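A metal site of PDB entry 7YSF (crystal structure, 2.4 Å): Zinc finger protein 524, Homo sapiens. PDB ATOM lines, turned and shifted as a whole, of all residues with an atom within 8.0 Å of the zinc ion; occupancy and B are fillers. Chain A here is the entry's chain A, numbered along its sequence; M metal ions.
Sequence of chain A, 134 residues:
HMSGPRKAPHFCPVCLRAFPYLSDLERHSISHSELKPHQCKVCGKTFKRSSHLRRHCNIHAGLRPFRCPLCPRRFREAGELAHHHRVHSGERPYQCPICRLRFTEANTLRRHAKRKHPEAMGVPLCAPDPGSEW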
ATOM      1  N   GLN A  95     -14.803  12.402   9.354  1.00  0.00           N
ATOM      2  CA  GLN A  95     -14.134  11.296  10.015  1.00  0.00           C
ATOM      3  C   GLN A  95     -14.705   9.966   9.533  1.00  0.00           C
ATOM      4  O   GLN A  95     -15.929   9.797   9.506  1.00  0.00           O
ATOM      5  CB  GLN A  95     -14.268  11.400  11.543  1.00  0.00           C
ATOM      6  CG  GLN A  95     -13.566  10.297  12.295  1.00  0.00           C
ATOM      7  CD  GLN A  95     -13.708  10.423  13.795  1.00  0.00           C
ATOM      8  OE1 GLN A  95     -12.806  10.060  14.548  1.00  0.00           O
ATOM      9  NE2 GLN A  95     -14.856  10.924  14.242  1.00  0.00           N
ATOM     10  N   CYS A  96     -13.828   9.058   9.156  1.00  0.00           N
ATOM     11  CA  CYS A  96     -14.264   7.723   8.762  1.00  0.00           C
ATOM     12  C   CYS A  96     -14.748   6.957   9.983  1.00  0.00           C
ATOM     13  O   CYS A  96     -14.007   6.865  10.975  1.00  0.00           O
ATOM     14  CB  CYS A  96     -13.141   6.961   8.075  1.00  0.00           C
ATOM     15  SG  CYS A  96     -13.533   5.238   7.705  1.00  0.00           S
ATOM     16  N   PRO A  97     -15.956   6.397   9.969  1.00  0.00           N
ATOM     17  CA  PRO A  97     -16.452   5.683  11.161  1.00  0.00           C
ATOM     18  C   PRO A  97     -15.702   4.391  11.443  1.00  0.00           C
ATOM     19  O   PRO A  97     -15.771   3.901  12.577  1.00  0.00           O
ATOM     20  CB  PRO A  97     -17.922   5.422  10.821  1.00  0.00           C
ATOM     21  CG  PRO A  97     -17.950   5.403   9.319  1.00  0.00           C
ATOM     22  CD  PRO A  97     -16.951   6.423   8.887  1.00  0.00           C
ATOM     23  N   ILE A  98     -15.014   3.832  10.457  1.00  0.00           N
ATOM     24  CA  ILE A  98     -14.348   2.545  10.599  1.00  0.00           C
ATOM     25  C   ILE A  98     -12.917   2.759  11.076  1.00  0.00           C
ATOM     26  O   ILE A  98     -12.528   2.248  12.128  1.00  0.00           O
ATOM     27  CB  ILE A  98     -14.367   1.754   9.279  1.00  0.00           C
ATOM     28  CG1 ILE A  98     -15.796   1.354   8.929  1.00  0.00           C
ATOM     29  CG2 ILE A  98     -13.469   0.524   9.376  1.00  0.00           C
ATOM     30  CD1 ILE A  98     -15.937   0.703   7.570  1.00  0.00           C
ATOM     31  N   CYS A  99     -12.115   3.505  10.317  1.00  0.00           N
ATOM     32  CA  CYS A  99     -10.718   3.658  10.690  1.00  0.00           C
ATOM     33  C   CYS A  99     -10.455   4.852  11.590  1.00  0.00           C
ATOM     34  O   CYS A  99      -9.340   4.972  12.104  1.00  0.00           O
ATOM     35  CB  CYS A  99      -9.825   3.732   9.445  1.00  0.00           C
ATOM     36  SG  CYS A  99      -9.845   5.336   8.641  1.00  0.00           S
ATOM     37  N   ARG A 100     -11.442   5.736  11.773  1.00  0.00           N
ATOM     38  CA  ARG A 100     -11.385   6.905  12.640  1.00  0.00           C
ATOM     39  C   ARG A 100     -10.402   7.970  12.152  1.00  0.00           C
ATOM     40  O   ARG A 100     -10.077   8.880  12.911  1.00  0.00           O
ATOM     41  CB  ARG A 100     -11.056   6.541  14.095  1.00  0.00           C
ATOM     42  CG  ARG A 100     -12.236   5.930  14.840  1.00  0.00           C
ATOM     43  CD  ARG A 100     -12.087   6.063  16.361  1.00  0.00           C
ATOM     44  NE  ARG A 100     -12.234   7.431  16.834  1.00  0.00           N
ATOM     45  CZ  ARG A 100     -13.379   8.114  16.835  1.00  0.00           C
ATOM     46  NH1 ARG A 100     -14.498   7.556  16.388  1.00  0.00           N
ATOM     47  NH2 ARG A 100     -13.408   9.368  17.288  1.00  0.00           N
ATOM     48  N   LEU A 101      -9.931   7.877  10.912  1.00  0.00           N
ATOM     49  CA  LEU A 101      -9.110   8.943  10.348  1.00  0.00           C
ATOM     50  C   LEU A 101      -9.982  10.131   9.971  1.00  0.00           C
ATOM     51  O   LEU A 101     -11.161   9.984   9.628  1.00  0.00           O
ATOM     52  CB  LEU A 101      -8.329   8.448   9.124  1.00  0.00           C
ATOM     53  CG  LEU A 101      -7.225   7.416   9.361  1.00  0.00           C
ATOM     54  CD1 LEU A 101      -6.606   6.993   8.033  1.00  0.00           C
ATOM     55  CD2 LEU A 101      -6.163   7.934  10.317  1.00  0.00           C
ATOM     56  N   ARG A 102      -9.397  11.318  10.047  1.00  0.00           N
ATOM     57  CA  ARG A 102     -10.107  12.563   9.781  1.00  0.00           C
ATOM     58  C   ARG A 102      -9.581  13.185   8.493  1.00  0.00           C
ATOM     59  O   ARG A 102      -8.376  13.151   8.225  1.00  0.00           O
ATOM     60  CB  ARG A 102      -9.944  13.537  10.942  1.00  0.00           C
ATOM     61  CG  ARG A 102     -10.633  13.087  12.224  1.00  0.00           C
ATOM     62  CD  ARG A 102     -10.914  14.257  13.148  1.00  0.00           C
ATOM     63  NE  ARG A 102     -12.273  14.209  13.681  1.00  0.00           N
ATOM     64  CZ  ARG A 102     -12.590  13.731  14.873  1.00  0.00           C
ATOM     65  NH1 ARG A 102     -11.652  13.247  15.678  1.00  0.00           N
ATOM     66  NH2 ARG A 102     -13.860  13.735  15.276  1.00  0.00           N
ATOM     67  N   PHE A 103     -10.490  13.751   7.698  1.00  0.00           N
ATOM     68  CA  PHE A 103     -10.152  14.268   6.382  1.00  0.00           C
ATOM     69  C   PHE A 103     -10.703  15.673   6.213  1.00  0.00           C
ATOM     70  O   PHE A 103     -11.716  16.048   6.812  1.00  0.00           O
ATOM     71  CB  PHE A 103     -10.710  13.354   5.284  1.00  0.00           C
ATOM     72  CG  PHE A 103     -10.162  11.953   5.340  1.00  0.00           C
ATOM     73  CD1 PHE A 103      -8.950  11.644   4.757  1.00  0.00           C
ATOM     74  CD2 PHE A 103     -10.865  10.947   5.990  1.00  0.00           C
ATOM     75  CE1 PHE A 103      -8.443  10.362   4.814  1.00  0.00           C
ATOM     76  CE2 PHE A 103     -10.363   9.657   6.043  1.00  0.00           C
ATOM     77  CZ  PHE A 103      -9.152   9.365   5.455  1.00  0.00           C
ATOM     78  N   LEU A 109     -12.813  11.749   2.022  1.00  0.00           N
ATOM     79  CA  LEU A 109     -13.328  10.662   2.849  1.00  0.00           C
ATOM     80  C   LEU A 109     -14.107   9.639   2.017  1.00  0.00           C
ATOM     81  O   LEU A 109     -14.004   8.435   2.266  1.00  0.00           O
ATOM     82  CB  LEU A 109     -14.210  11.231   3.968  1.00  0.00           C
ATOM     83  CG  LEU A 109     -15.099  10.243   4.711  1.00  0.00           C
ATOM     84  CD1 LEU A 109     -14.258   9.224   5.466  1.00  0.00           C
ATOM     85  CD2 LEU A 109     -16.041  10.958   5.655  1.00  0.00           C
ATOM     86  N   HIS A 112     -11.755   7.582   0.241  1.00  0.00           N
ATOM     87  CA  HIS A 112     -11.089   6.737   1.213  1.00  0.00           C
ATOM     88  C   HIS A 112     -11.948   5.520   1.565  1.00  0.00           C
ATOM     89  O   HIS A 112     -11.443   4.403   1.657  1.00  0.00           O
ATOM     90  CB  HIS A 112     -10.756   7.542   2.474  1.00  0.00           C
ATOM     91  CG  HIS A 112     -10.429   6.695   3.660  1.00  0.00           C
ATOM     92  ND1 HIS A 112      -9.159   6.206   3.906  1.00  0.00           N
ATOM     93  CD2 HIS A 112     -11.196   6.244   4.678  1.00  0.00           C
ATOM     94  CE1 HIS A 112      -9.163   5.504   5.018  1.00  0.00           C
ATOM     95  NE2 HIS A 112     -10.389   5.509   5.505  1.00  0.00           N
ATOM     96  N   ALA A 113     -13.254   5.741   1.763  1.00  0.00           N
ATOM     97  CA  ALA A 113     -14.135   4.639   2.145  1.00  0.00           C
ATOM     98  C   ALA A 113     -14.194   3.574   1.049  1.00  0.00           C
ATOM     99  O   ALA A 113     -14.072   2.383   1.322  1.00  0.00           O
ATOM    100  CB  ALA A 113     -15.541   5.174   2.451  1.00  0.00           C
ATOM    101  N   LYS A 114     -14.375   4.000  -0.206  1.00  0.00           N
ATOM    102  CA  LYS A 114     -14.529   3.046  -1.299  1.00  0.00           C
ATOM    103  C   LYS A 114     -13.227   2.300  -1.591  1.00  0.00           C
ATOM    104  O   LYS A 114     -13.264   1.177  -2.103  1.00  0.00           O
ATOM    105  CB  LYS A 114     -15.035   3.761  -2.543  1.00  0.00           C
ATOM    106  CG  LYS A 114     -16.261   4.618  -2.292  1.00  0.00           C
ATOM    107  CD  LYS A 114     -16.576   5.502  -3.483  1.00  0.00           C
ATOM    108  CE  LYS A 114     -16.877   4.674  -4.719  1.00  0.00           C
ATOM    109  NZ  LYS A 114     -17.973   3.690  -4.463  1.00  0.00           N
ATOM    110  N   LYS A 116     -10.561   1.882   0.873  1.00  0.00           N
ATOM    111  CA  LYS A 116     -10.049   1.206   2.068  1.00  0.00           C
ATOM    112  C   LYS A 116     -11.078   0.327   2.753  1.00  0.00           C
ATOM    113  O   LYS A 116     -10.684  -0.610   3.460  1.00  0.00           O
ATOM    114  CB  LYS A 116      -9.516   2.236   3.070  1.00  0.00           C
ATOM    115  CG  LYS A 116      -8.641   3.306   2.447  1.00  0.00           C
ATOM    116  CD  LYS A 116      -7.337   2.742   1.925  1.00  0.00           C
ATOM    117  CE  LYS A 116      -6.552   2.072   3.032  1.00  0.00           C
ATOM    118  NZ  LYS A 116      -5.524   1.144   2.493  1.00  0.00           N
ATOM    119  N   HIS A 117     -12.371   0.588   2.575  1.00  0.00           N
ATOM    120  CA  HIS A 117     -13.422  -0.222   3.191  1.00  0.00           C
ATOM    121  C   HIS A 117     -14.462  -0.606   2.150  1.00  0.00           C
ATOM    122  O   HIS A 117     -15.615  -0.166   2.207  1.00  0.00           O
ATOM    123  CB  HIS A 117     -14.070   0.541   4.344  1.00  0.00           C
ATOM    124  CG  HIS A 117     -13.099   1.293   5.184  1.00  0.00           C
ATOM    125  ND1 HIS A 117     -12.243   0.673   6.075  1.00  0.00           N
ATOM    126  CD2 HIS A 117     -12.819   2.616   5.260  1.00  0.00           C
ATOM    127  CE1 HIS A 117     -11.490   1.580   6.669  1.00  0.00           C
ATOM    128  NE2 HIS A 117     -11.816   2.771   6.193  1.00  0.00           N
ATOM    129  N   MET A 121     -19.327   1.832   3.831  1.00  0.00           N
ATOM    130  CA  MET A 121     -19.018   2.732   4.943  1.00  0.00           C
ATOM    131  C   MET A 121     -19.930   3.948   4.903  1.00  0.00           C
ATOM    132  O   MET A 121     -19.498   5.065   5.159  1.00  0.00           O
ATOM    133  CB  MET A 121     -17.554   3.168   4.900  1.00  0.00           C
HETATM  134 ZN    ZN M   1     -11.340   4.455   7.141  1.00  0.00          ZN
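Of the 16 residues printed, 4 come within 4 Å of the zinc ion.
A ring nitrogen (NE2) of His 117 binds the zinc ion (2.0 Å).
NE2 of His 112 binds the zinc ion, at 2.2 Å.
SG of Cys 99 binds the zinc ion, at 2.3 Å.
The zinc ion is bound by SG of Cys 96 (2.4 Å).
SG of Cys 99 sits close to N of Leu 101 (3.4 Å).
The backbone NH of Ile 98 lies close to the side-chain sulfur of Cys 96, 3.4 Å away.
The backbone NH (N) of Cys 96 sits at hydrogen-bond distance from the backbone carbonyl oxygen (O) of Leu 101.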
